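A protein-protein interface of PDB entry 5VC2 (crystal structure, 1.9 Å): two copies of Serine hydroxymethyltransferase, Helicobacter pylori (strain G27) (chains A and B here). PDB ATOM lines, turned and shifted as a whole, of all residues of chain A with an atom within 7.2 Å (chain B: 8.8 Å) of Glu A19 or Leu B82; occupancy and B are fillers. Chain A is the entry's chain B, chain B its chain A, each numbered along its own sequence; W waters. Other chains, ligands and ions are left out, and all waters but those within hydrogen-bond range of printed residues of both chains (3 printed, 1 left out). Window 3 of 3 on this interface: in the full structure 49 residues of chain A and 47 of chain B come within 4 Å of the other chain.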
ATOM      1  N   LEU A  13      14.781   6.654  13.325  1.00  0.00           N
ATOM      2  CA  LEU A  13      15.146   5.598  14.272  1.00  0.00           C
ATOM      3  C   LEU A  13      16.404   5.951  15.049  1.00  0.00           C
ATOM      4  O   LEU A  13      16.518   5.632  16.239  1.00  0.00           O
ATOM      5  CB  LEU A  13      15.348   4.270  13.535  1.00  0.00           C
ATOM      6  CG  LEU A  13      14.110   3.518  13.055  1.00  0.00           C
ATOM      7  CD1 LEU A  13      14.504   2.325  12.186  1.00  0.00           C
ATOM      8  CD2 LEU A  13      13.324   3.040  14.266  1.00  0.00           C
ATOM      9  N   GLU A  14      17.375   6.587  14.391  1.00  0.00           N
ATOM     10  CA  GLU A  14      18.591   6.968  15.092  1.00  0.00           C
ATOM     11  C   GLU A  14      18.274   7.845  16.293  1.00  0.00           C
ATOM     12  O   GLU A  14      18.951   7.762  17.322  1.00  0.00           O
ATOM     13  CB  GLU A  14      19.541   7.682  14.134  1.00  0.00           C
ATOM     14  CG  GLU A  14      20.978   7.666  14.578  1.00  0.00           C
ATOM     15  CD  GLU A  14      21.902   8.110  13.479  1.00  0.00           C
ATOM     16  OE1 GLU A  14      21.385   8.510  12.415  1.00  0.00           O
ATOM     17  OE2 GLU A  14      23.135   8.054  13.677  1.00  0.00           O
ATOM     18  N   THR A  16      14.847   8.096  17.666  1.00  0.00           N
ATOM     19  CA  THR A  16      13.684   7.655  18.432  1.00  0.00           C
ATOM     20  C   THR A  16      13.794   6.245  18.999  1.00  0.00           C
ATOM     21  O   THR A  16      13.034   5.913  19.912  1.00  0.00           O
ATOM     22  CB  THR A  16      12.418   7.721  17.568  1.00  0.00           C
ATOM     23  OG1 THR A  16      12.491   6.720  16.542  1.00  0.00           O
ATOM     24  CG2 THR A  16      12.284   9.099  16.916  1.00  0.00           C
ATOM     25  N   ASP A  17      14.693   5.401  18.483  1.00  0.00           N
ATOM     26  CA  ASP A  17      14.759   3.992  18.902  1.00  0.00           C
ATOM     27  C   ASP A  17      16.198   3.518  18.689  1.00  0.00           C
ATOM     28  O   ASP A  17      16.516   2.760  17.759  1.00  0.00           O
ATOM     29  CB  ASP A  17      13.755   3.129  18.131  1.00  0.00           C
ATOM     30  CG  ASP A  17      13.545   1.760  18.757  1.00  0.00           C
ATOM     31  OD1 ASP A  17      14.397   1.293  19.547  1.00  0.00           O
ATOM     32  OD2 ASP A  17      12.509   1.153  18.468  1.00  0.00           O
ATOM     33  N   SER A  18      17.086   3.989  19.572  1.00  0.00           N
ATOM     34  CA  SER A  18      18.507   3.701  19.423  1.00  0.00           C
ATOM     35  C   SER A  18      18.772   2.208  19.475  1.00  0.00           C
ATOM     36  O   SER A  18      19.741   1.725  18.884  1.00  0.00           O
ATOM     37  CB  SER A  18      19.309   4.411  20.518  1.00  0.00           C
ATOM     38  OG  SER A  18      19.162   5.824  20.458  1.00  0.00           O
ATOM     39  N   GLU A  19      17.928   1.466  20.192  1.00  0.00           N
ATOM     40  CA  GLU A  19      18.161   0.038  20.356  1.00  0.00           C
ATOM     41  C   GLU A  19      17.950  -0.696  19.040  1.00  0.00           C
ATOM     42  O   GLU A  19      18.760  -1.545  18.653  1.00  0.00           O
ATOM     43  CB  GLU A  19      17.235  -0.510  21.445  1.00  0.00           C
ATOM     44  CG  GLU A  19      17.550  -1.932  21.892  1.00  0.00           C
ATOM     45  CD  GLU A  19      16.758  -2.348  23.130  1.00  0.00           C
ATOM     46  OE1 GLU A  19      17.112  -3.379  23.731  1.00  0.00           O
ATOM     47  OE2 GLU A  19      15.788  -1.647  23.501  1.00  0.00           O
ATOM     48  N   ILE A  20      16.864  -0.387  18.337  1.00  0.00           N
ATOM     49  CA  ILE A  20      16.650  -0.998  17.028  1.00  0.00           C
ATOM     50  C   ILE A  20      17.675  -0.476  16.026  1.00  0.00           C
ATOM     51  O   ILE A  20      18.214  -1.236  15.212  1.00  0.00           O
ATOM     52  CB  ILE A  20      15.206  -0.754  16.553  1.00  0.00           C
ATOM     53  CG1 ILE A  20      14.236  -1.713  17.252  1.00  0.00           C
ATOM     54  CG2 ILE A  20      15.093  -0.922  15.044  1.00  0.00           C
ATOM     55  CD1 ILE A  20      14.380  -3.175  16.817  1.00  0.00           C
ATOM     56  N   PHE A  21      17.969   0.825  16.069  1.00  0.00           N
ATOM     57  CA  PHE A  21      18.941   1.385  15.137  1.00  0.00           C
ATOM     58  C   PHE A  21      20.298   0.707  15.284  1.00  0.00           C
ATOM     59  O   PHE A  21      20.954   0.394  14.284  1.00  0.00           O
ATOM     60  CB  PHE A  21      19.092   2.892  15.341  1.00  0.00           C
ATOM     61  CG  PHE A  21      20.091   3.513  14.412  1.00  0.00           C
ATOM     62  CD1 PHE A  21      19.724   3.868  13.124  1.00  0.00           C
ATOM     63  CD2 PHE A  21      21.407   3.701  14.805  1.00  0.00           C
ATOM     64  CE1 PHE A  21      20.645   4.426  12.256  1.00  0.00           C
ATOM     65  CE2 PHE A  21      22.330   4.252  13.942  1.00  0.00           C
ATOM     66  CZ  PHE A  21      21.949   4.614  12.665  1.00  0.00           C
ATOM     67  N   GLU A  22      20.750   0.500  16.524  1.00  0.00           N
ATOM     68  CA  GLU A  22      21.997  -0.231  16.727  1.00  0.00           C
ATOM     69  C   GLU A  22      21.940  -1.627  16.110  1.00  0.00           C
ATOM     70  O   GLU A  22      22.933  -2.106  15.546  1.00  0.00           O
ATOM     71  CB  GLU A  22      22.316  -0.322  18.222  1.00  0.00           C
ATOM     72  CG  GLU A  22      23.222  -1.476  18.533  1.00  0.00           C
ATOM     73  CD  GLU A  22      24.157  -1.213  19.686  1.00  0.00           C
ATOM     74  OE1 GLU A  22      23.941  -0.233  20.435  1.00  0.00           O
ATOM     75  OE2 GLU A  22      25.126  -1.990  19.822  1.00  0.00           O
ATOM     76  N   LEU A  23      20.805  -2.317  16.234  1.00  0.00           N
ATOM     77  CA  LEU A  23      20.728  -3.666  15.672  1.00  0.00           C
ATOM     78  C   LEU A  23      20.763  -3.631  14.147  1.00  0.00           C
ATOM     79  O   LEU A  23      21.348  -4.516  13.512  1.00  0.00           O
ATOM     80  CB  LEU A  23      19.472  -4.377  16.164  1.00  0.00           C
ATOM     81  CG  LEU A  23      19.442  -4.681  17.664  1.00  0.00           C
ATOM     82  CD1 LEU A  23      18.027  -5.013  18.123  1.00  0.00           C
ATOM     83  CD2 LEU A  23      20.398  -5.821  18.003  1.00  0.00           C
ATOM     84  N   ILE A  24      20.142  -2.622  13.537  1.00  0.00           N
ATOM     85  CA  ILE A  24      20.232  -2.483  12.083  1.00  0.00           C
ATOM     86  C   ILE A  24      21.674  -2.216  11.673  1.00  0.00           C
ATOM     87  O   ILE A  24      22.199  -2.822  10.728  1.00  0.00           O
ATOM     88  CB  ILE A  24      19.290  -1.368  11.593  1.00  0.00           C
ATOM     89  CG1 ILE A  24      17.834  -1.769  11.798  1.00  0.00           C
ATOM     90  CG2 ILE A  24      19.578  -1.001  10.127  1.00  0.00           C
ATOM     91  CD1 ILE A  24      16.851  -0.604  11.607  1.00  0.00           C
ATOM     92  N   VAL B  76      16.914 -17.668  18.301  1.00  0.00           N
ATOM     93  CA  VAL B  76      16.065 -16.495  18.110  1.00  0.00           C
ATOM     94  C   VAL B  76      16.948 -15.273  17.908  1.00  0.00           C
ATOM     95  O   VAL B  76      17.830 -14.993  18.727  1.00  0.00           O
ATOM     96  CB  VAL B  76      15.111 -16.271  19.301  1.00  0.00           C
ATOM     97  CG1 VAL B  76      14.207 -15.071  19.043  1.00  0.00           C
ATOM     98  CG2 VAL B  76      14.281 -17.517  19.566  1.00  0.00           C
ATOM     99  N   ASP B  77      16.701 -14.542  16.824  1.00  0.00           N
ATOM    100  CA  ASP B  77      17.388 -13.283  16.582  1.00  0.00           C
ATOM    101  C   ASP B  77      17.111 -12.296  17.715  1.00  0.00           C
ATOM    102  O   ASP B  77      16.008 -12.262  18.272  1.00  0.00           O
ATOM    103  CB  ASP B  77      16.923 -12.709  15.244  1.00  0.00           C
ATOM    104  CG  ASP B  77      17.840 -11.632  14.717  1.00  0.00           C
ATOM    105  OD1 ASP B  77      17.773 -10.492  15.211  1.00  0.00           O
ATOM    106  OD2 ASP B  77      18.642 -11.933  13.813  1.00  0.00           O
ATOM    107  N   LYS B  78      18.126 -11.501  18.072  1.00  0.00           N
ATOM    108  CA  LYS B  78      17.917 -10.437  19.052  1.00  0.00           C
ATOM    109  C   LYS B  78      16.742  -9.553  18.677  1.00  0.00           C
ATOM    110  O   LYS B  78      16.028  -9.061  19.556  1.00  0.00           O
ATOM    111  CB  LYS B  78      19.158  -9.555  19.186  1.00  0.00           C
ATOM    112  CG  LYS B  78      20.281 -10.131  20.023  1.00  0.00           C
ATOM    113  CD  LYS B  78      21.309  -9.049  20.302  1.00  0.00           C
ATOM    114  CE  LYS B  78      22.633  -9.621  20.775  1.00  0.00           C
ATOM    115  NZ  LYS B  78      23.706  -8.578  20.745  1.00  0.00           N
ATOM    116  N   ILE B  79      16.529  -9.333  17.380  1.00  0.00           N
ATOM    117  CA  ILE B  79      15.448  -8.451  16.959  1.00  0.00           C
ATOM    118  C   ILE B  79      14.095  -9.048  17.320  1.00  0.00           C
ATOM    119  O   ILE B  79      13.196  -8.337  17.774  1.00  0.00           O
ATOM    120  CB  ILE B  79      15.555  -8.154  15.456  1.00  0.00           C
ATOM    121  CG1 ILE B  79      16.762  -7.257  15.195  1.00  0.00           C
ATOM    122  CG2 ILE B  79      14.250  -7.532  14.947  1.00  0.00           C
ATOM    123  CD1 ILE B  79      17.355  -7.411  13.813  1.00  0.00           C
ATOM    124  N   GLU B  80      13.928 -10.361  17.145  1.00  0.00           N
ATOM    125  CA  GLU B  80      12.654 -10.972  17.508  1.00  0.00           C
ATOM    126  C   GLU B  80      12.468 -11.015  19.027  1.00  0.00           C
ATOM    127  O   GLU B  80      11.359 -10.790  19.529  1.00  0.00           O
ATOM    128  CB  GLU B  80      12.538 -12.370  16.909  1.00  0.00           C
ATOM    129  CG  GLU B  80      11.174 -13.001  17.201  1.00  0.00           C
ATOM    130  CD  GLU B  80      11.014 -14.367  16.572  1.00  0.00           C
ATOM    131  OE1 GLU B  80      11.954 -14.813  15.882  1.00  0.00           O
ATOM    132  OE2 GLU B  80       9.952 -14.996  16.772  1.00  0.00           O
ATOM    133  N   SER B  81      13.544 -11.285  19.773  1.00  0.00           N
ATOM    134  CA  SER B  81      13.442 -11.245  21.229  1.00  0.00           C
ATOM    135  C   SER B  81      13.012  -9.864  21.702  1.00  0.00           C
ATOM    136  O   SER B  81      12.199  -9.742  22.626  1.00  0.00           O
ATOM    137  CB  SER B  81      14.775 -11.638  21.865  1.00  0.00           C
ATOM    138  OG  SER B  81      15.190 -12.911  21.414  1.00  0.00           O
ATOM    139  N   LEU B  82      13.538  -8.808  21.064  1.00  0.00           N
ATOM    140  CA  LEU B  82      13.158  -7.451  21.444  1.00  0.00           C
ATOM    141  C   LEU B  82      11.692  -7.169  21.123  1.00  0.00           C
ATOM    142  O   LEU B  82      10.992  -6.528  21.916  1.00  0.00           O
ATOM    143  CB  LEU B  82      14.065  -6.436  20.746  1.00  0.00           C
ATOM    144  CG  LEU B  82      13.891  -4.982  21.200  1.00  0.00           C
ATOM    145  CD1 LEU B  82      14.150  -4.866  22.722  1.00  0.00           C
ATOM    146  CD2 LEU B  82      14.822  -4.059  20.419  1.00  0.00           C
ATOM    147  N   ALA B  83      11.214  -7.611  19.953  1.00  0.00           N
ATOM    148  CA  ALA B  83       9.800  -7.447  19.628  1.00  0.00           C
ATOM    149  C   ALA B  83       8.913  -8.150  20.650  1.00  0.00           C
ATOM    150  O   ALA B  83       7.863  -7.622  21.048  1.00  0.00           O
ATOM    151  CB  ALA B  83       9.515  -7.987  18.220  1.00  0.00           C
ATOM    152  N   ILE B  84       9.315  -9.353  21.072  1.00  0.00           N
ATOM    153  CA  ILE B  84       8.540 -10.126  22.042  1.00  0.00           C
ATOM    154  C   ILE B  84       8.554  -9.443  23.402  1.00  0.00           C
ATOM    155  O   ILE B  84       7.511  -9.318  24.068  1.00  0.00           O
ATOM    156  CB  ILE B  84       9.091 -11.561  22.109  1.00  0.00           C
ATOM    157  CG1 ILE B  84       8.715 -12.326  20.835  1.00  0.00           C
ATOM    158  CG2 ILE B  84       8.598 -12.304  23.365  1.00  0.00           C
ATOM    159  CD1 ILE B  84       9.456 -13.641  20.680  1.00  0.00           C
ATOM    160  N   GLU B  85       9.734  -8.991  23.834  1.00  0.00           N
ATOM    161  CA  GLU B  85       9.866  -8.293  25.108  1.00  0.00           C
ATOM    162  C   GLU B  85       8.980  -7.049  25.148  1.00  0.00           C
ATOM    163  O   GLU B  85       8.256  -6.814  26.126  1.00  0.00           O
ATOM    164  CB  GLU B  85      11.339  -7.937  25.339  1.00  0.00           C
ATOM    165  CG  GLU B  85      11.614  -7.029  26.516  1.00  0.00           C
ATOM    166  CD  GLU B  85      13.029  -6.456  26.486  1.00  0.00           C
ATOM    167  OE1 GLU B  85      13.982  -7.224  26.224  1.00  0.00           O
ATOM    168  OE2 GLU B  85      13.183  -5.234  26.705  1.00  0.00           O
ATOM    169  N   ARG B  86       9.015  -6.244  24.086  1.00  0.00           N
ATOM    170  CA  ARG B  86       8.190  -5.039  24.051  1.00  0.00           C
ATOM    171  C   ARG B  86       6.706  -5.382  24.010  1.00  0.00           C
ATOM    172  O   ARG B  86       5.893  -4.728  24.680  1.00  0.00           O
ATOM    173  CB  ARG B  86       8.599  -4.168  22.857  1.00  0.00           C
ATOM    174  CG  ARG B  86      10.007  -3.570  23.044  1.00  0.00           C
ATOM    175  CD  ARG B  86      10.422  -2.720  21.837  1.00  0.00           C
ATOM    176  NE  ARG B  86      11.718  -2.073  22.030  1.00  0.00           N
ATOM    177  CZ  ARG B  86      12.342  -1.369  21.094  1.00  0.00           C
ATOM    178  NH1 ARG B  86      11.776  -1.219  19.886  1.00  0.00           N
ATOM    179  NH2 ARG B  86      13.516  -0.797  21.367  1.00  0.00           N
ATOM    180  N   ALA B  87       6.337  -6.425  23.261  1.00  0.00           N
ATOM    181  CA  ALA B  87       4.947  -6.867  23.232  1.00  0.00           C
ATOM    182  C   ALA B  87       4.474  -7.296  24.618  1.00  0.00           C
ATOM    183  O   ALA B  87       3.372  -6.941  25.042  1.00  0.00           O
ATOM    184  CB  ALA B  87       4.780  -8.018  22.241  1.00  0.00           C
ATOM    185  N   LYS B  88       5.280  -8.095  25.321  1.00  0.00           N
ATOM    186  CA  LYS B  88       4.869  -8.548  26.649  1.00  0.00           C
ATOM    187  C   LYS B  88       4.609  -7.361  27.570  1.00  0.00           C
ATOM    188  O   LYS B  88       3.631  -7.353  28.325  1.00  0.00           O
ATOM    189  CB  LYS B  88       5.932  -9.474  27.234  1.00  0.00           C
ATOM    190  CG  LYS B  88       6.008 -10.833  26.525  1.00  0.00           C
ATOM    191  CD  LYS B  88       7.298 -11.543  26.812  1.00  0.00           C
ATOM    192  CE  LYS B  88       7.485 -11.811  28.291  1.00  0.00           C
ATOM    193  NZ  LYS B  88       8.768 -12.553  28.536  1.00  0.00           N
ATOM    194  N   LYS B  89       5.445  -6.324  27.489  1.00  0.00           N
ATOM    195  CA  LYS B  89       5.209  -5.135  28.307  1.00  0.00           C
ATOM    196  C   LYS B  89       3.962  -4.376  27.841  1.00  0.00           C
ATOM    197  O   LYS B  89       3.117  -3.984  28.659  1.00  0.00           O
ATOM    198  CB  LYS B  89       6.431  -4.220  28.276  1.00  0.00           C
ATOM    199  CG  LYS B  89       6.360  -3.141  29.354  1.00  0.00           C
ATOM    200  CD  LYS B  89       7.522  -2.169  29.299  1.00  0.00           C
ATOM    201  CE  LYS B  89       7.285  -1.003  30.252  1.00  0.00           C
ATOM    202  NZ  LYS B  89       7.153  -1.465  31.653  1.00  0.00           N
ATOM    203  N   ALA B  96       4.323 -13.867  24.006  1.00  0.00           N
ATOM    204  CA  ALA B  96       3.948 -13.250  22.740  1.00  0.00           C
ATOM    205  C   ALA B  96       4.546 -14.042  21.586  1.00  0.00           C
ATOM    206  O   ALA B  96       5.648 -14.594  21.693  1.00  0.00           O
ATOM    207  CB  ALA B  96       4.411 -11.793  22.649  1.00  0.00           C
ATOM    208  N   VAL B  98       5.119 -13.131  17.523  1.00  0.00           N
ATOM    209  CA  VAL B  98       5.045 -11.977  16.641  1.00  0.00           C
ATOM    210  C   VAL B  98       5.203 -12.375  15.174  1.00  0.00           C
ATOM    211  O   VAL B  98       5.504 -11.527  14.336  1.00  0.00           O
ATOM    212  CB  VAL B  98       6.085 -10.919  17.031  1.00  0.00           C
ATOM    213  CG1 VAL B  98       5.839 -10.406  18.466  1.00  0.00           C
ATOM    214  CG2 VAL B  98       7.486 -11.497  16.875  1.00  0.00           C
ATOM    215  N   MET B 269      12.893 -10.243   8.935  1.00  0.00           N
ATOM    216  CA  MET B 269      13.467  -9.503  10.058  1.00  0.00           C
ATOM    217  C   MET B 269      13.140  -8.020  10.001  1.00  0.00           C
ATOM    218  O   MET B 269      13.007  -7.380  11.048  1.00  0.00           O
ATOM    219  CB  MET B 269      14.983  -9.702  10.123  1.00  0.00           C
ATOM    220  CG  MET B 269      15.422 -11.111  10.479  1.00  0.00           C
ATOM    221  SD  MET B 269      14.465 -11.848  11.826  1.00  0.00           S
ATOM    222  CE  MET B 269      14.692 -10.663  13.127  1.00  0.00           C
ATOM    223  N   ILE B 272       9.627  -7.832  11.580  1.00  0.00           N
ATOM    224  CA  ILE B 272       9.675  -8.023  13.034  1.00  0.00           C
ATOM    225  C   ILE B 272      10.289  -6.806  13.713  1.00  0.00           C
ATOM    226  O   ILE B 272       9.781  -6.326  14.731  1.00  0.00           O
ATOM    227  CB  ILE B 272      10.435  -9.316  13.366  1.00  0.00           C
ATOM    228  CG1 ILE B 272       9.642 -10.517  12.841  1.00  0.00           C
ATOM    229  CG2 ILE B 272      10.705  -9.427  14.889  1.00  0.00           C
ATOM    230  CD1 ILE B 272      10.315 -11.838  13.087  1.00  0.00           C
ATOM    231  N   ALA B 273      11.382  -6.271  13.155  1.00  0.00           N
ATOM    232  CA  ALA B 273      11.917  -5.011  13.677  1.00  0.00           C
ATOM    233  C   ALA B 273      10.875  -3.901  13.640  1.00  0.00           C
ATOM    234  O   ALA B 273      10.744  -3.128  14.602  1.00  0.00           O
ATOM    235  CB  ALA B 273      13.156  -4.587  12.890  1.00  0.00           C
ATOM    236  N   LYS B 275       7.653  -4.146  13.793  1.00  0.00           N
ATOM    237  CA  LYS B 275       6.690  -4.349  14.881  1.00  0.00           C
ATOM    238  C   LYS B 275       7.262  -3.882  16.212  1.00  0.00           C
ATOM    239  O   LYS B 275       6.561  -3.246  17.012  1.00  0.00           O
ATOM    240  CB  LYS B 275       6.288  -5.829  14.974  1.00  0.00           C
ATOM    241  CG  LYS B 275       5.411  -6.324  13.811  1.00  0.00           C
ATOM    242  CD  LYS B 275       5.049  -7.810  13.957  1.00  0.00           C
ATOM    243  CE  LYS B 275       4.150  -8.288  12.808  1.00  0.00           C
ATOM    244  NZ  LYS B 275       3.833  -9.765  12.870  1.00  0.00           N
ATOM    245  N   ALA B 276       8.534  -4.208  16.470  1.00  0.00           N
ATOM    246  CA  ALA B 276       9.196  -3.771  17.699  1.00  0.00           C
ATOM    247  C   ALA B 276       9.257  -2.252  17.796  1.00  0.00           C
ATOM    248  O   ALA B 276       9.043  -1.682  18.873  1.00  0.00           O
ATOM    249  CB  ALA B 276      10.600  -4.353  17.757  1.00  0.00           C
ATOM    250  N   VAL B 277       9.576  -1.587  16.680  1.00  0.00           N
ATOM    251  CA  VAL B 277       9.580  -0.128  16.620  1.00  0.00           C
ATOM    252  C   VAL B 277       8.210   0.422  16.988  1.00  0.00           C
ATOM    253  O   VAL B 277       8.089   1.381  17.768  1.00  0.00           O
ATOM    254  CB  VAL B 277      10.006   0.338  15.216  1.00  0.00           C
ATOM    255  CG1 VAL B 277       9.741   1.815  15.029  1.00  0.00           C
ATOM    256  CG2 VAL B 277      11.470   0.000  14.976  1.00  0.00           C
ATOM    257  N   PHE B 279       5.820  -1.024  18.734  1.00  0.00           N
ATOM    258  CA  PHE B 279       5.472  -1.299  20.129  1.00  0.00           C
ATOM    259  C   PHE B 279       6.099  -0.282  21.076  1.00  0.00           C
ATOM    260  O   PHE B 279       5.470   0.118  22.061  1.00  0.00           O
ATOM    261  CB  PHE B 279       5.897  -2.712  20.520  1.00  0.00           C
ATOM    262  CG  PHE B 279       5.188  -3.794  19.761  1.00  0.00           C
ATOM    263  CD1 PHE B 279       3.932  -3.575  19.207  1.00  0.00           C
ATOM    264  CD2 PHE B 279       5.781  -5.044  19.616  1.00  0.00           C
ATOM    265  CE1 PHE B 279       3.283  -4.591  18.497  1.00  0.00           C
ATOM    266  CE2 PHE B 279       5.151  -6.052  18.916  1.00  0.00           C
ATOM    267  CZ  PHE B 279       3.902  -5.829  18.349  1.00  0.00           C
ATOM    268  N   LYS B 280       7.335   0.156  20.795  1.00  0.00           N
ATOM    269  CA  LYS B 280       7.977   1.150  21.656  1.00  0.00           C
ATOM    270  C   LYS B 280       7.308   2.514  21.528  1.00  0.00           C
ATOM    271  O   LYS B 280       7.137   3.223  22.529  1.00  0.00           O
ATOM    272  CB  LYS B 280       9.472   1.257  21.338  1.00  0.00           C
ATOM    273  CG  LYS B 280      10.199   2.317  22.158  1.00  0.00           C
ATOM    274  CD  LYS B 280      11.666   2.401  21.785  1.00  0.00           C
ATOM    275  CE  LYS B 280      12.408   3.419  22.644  1.00  0.00           C
ATOM    276  NZ  LYS B 280      12.021   4.826  22.328  1.00  0.00           N
ATOM    277  N   LEU B 283       4.231   2.405  23.705  1.00  0.00           N
ATOM    278  CA  LEU B 283       4.453   2.505  25.146  1.00  0.00           C
ATOM    279  C   LEU B 283       4.591   3.942  25.636  1.00  0.00           C
ATOM    280  O   LEU B 283       4.529   4.174  26.852  1.00  0.00           O
ATOM    281  CB  LEU B 283       5.698   1.706  25.528  1.00  0.00           C
ATOM    282  CG  LEU B 283       5.579   0.180  25.453  1.00  0.00           C
ATOM    283  CD1 LEU B 283       6.966  -0.453  25.403  1.00  0.00           C
ATOM    284  CD2 LEU B 283       4.788  -0.373  26.655  1.00  0.00           C
HETATM  285  O   HOH W   1      12.780  -1.925  24.698  1.00  0.00           O
HETATM  286  O   HOH W   2      10.381   2.926  18.358  1.00  0.00           O
HETATM  287  O   HOH W   3      10.319   5.085  20.197  1.00  0.00           O
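The side-chain carboxylate (OD2) of Asp A17 lies within salt-bridge range of the guanidinium group (NH1) of Arg B86 (2.9 Å). OE2 of Glu A19 is in salt-bridge range of NH2 of Arg B86 (3.2 Å). The backbone carbonyl oxygen (O) of Thr A16 is in hydrogen-bond range of the side-chain amino group (NZ) of Lys B280, 2.8 Å away.
The backbone carbonyl oxygen (O) of Ala B276 sits at hydrogen-bond distance from the guanidinium group (NH1) of Arg B86, 3.0 Å away. The side-chain carboxylate (OD1) of Asp A17 is in hydrogen-bond range of the backbone NH (N) of Ile A20. N of Ile B79 is in hydrogen-bond range of OD1 of Asp B77 (2.8 Å).
Among the printed residues, merely in contact across the chains: Glu A19 with Leu B82 (3.5 Å), Asp A17 with Lys B280 (3.6 Å), Leu A13 with Val B277 (3.6 Å), Ile A20 with Arg B86 (3.6 Å), Asp A17 with Val B277 (3.7 Å), Ile A20 with Leu B82 (3.7 Å), Ile A20 with Val B277 (3.7 Å) and Leu A23 with Ile B79 (3.9 Å).
Glu A19 touches just these residues of chain B: Leu B82 (3.5 Å) and Arg B86 (3.2 Å). Leu B82 touches two residues of chain A. Ser A18 touches none of the printed residues of chain B. Of the printed residues of chain B, Thr A16 touches Lys B280 (2.8 Å). Printed residues of chain B within 4 Å of Leu A23: Ile B79 (3.9 Å). Printed residues of chain A within 4 Å of Val B277: Leu A13, Asp A17 and Ile A20. Of the printed residues of chain B, Leu A13 touches Val B277 (3.6 Å). Of the printed residues of chain A, Lys B280 touches Thr A16 (2.8 Å) and Asp A17 (3.6 Å). Val B76 touches none of the printed residues of chain A. Glu A22 touches none of the printed residues of chain B. The nearest residue of chain B that does not touch Glu A19 is Glu B85 (5.3 Å). The nearest residue of chain A that does not touch Leu B82 is Leu A23 (4.1 Å).
Hydrophobic or aromatic side chains of chain B within 4 Å of the printed part of chain A: Ile B79, Leu B82 and Val B277. Among the printed residues, Asp or Glu carboxylates within 4 Å of a Lys or Arg side-chain nitrogen of the other chain: Asp A17 with Arg B86 (2.9 Å) and Glu A19 with Arg B86 (3.2 Å).
No position is printed for both chains.
Water W3 bridges the side-chain amino group of Lys B280 (2.7 Å) and the backbone carbonyl oxygen of Thr A16 (2.9 Å). Water W2 bridges OD2 of Asp A17 and O of Val B277. Water W1 lies within hydrogen-bond range of NE of Arg B86 (2.9 Å) and OE2 of Glu A19 (3.2 Å).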
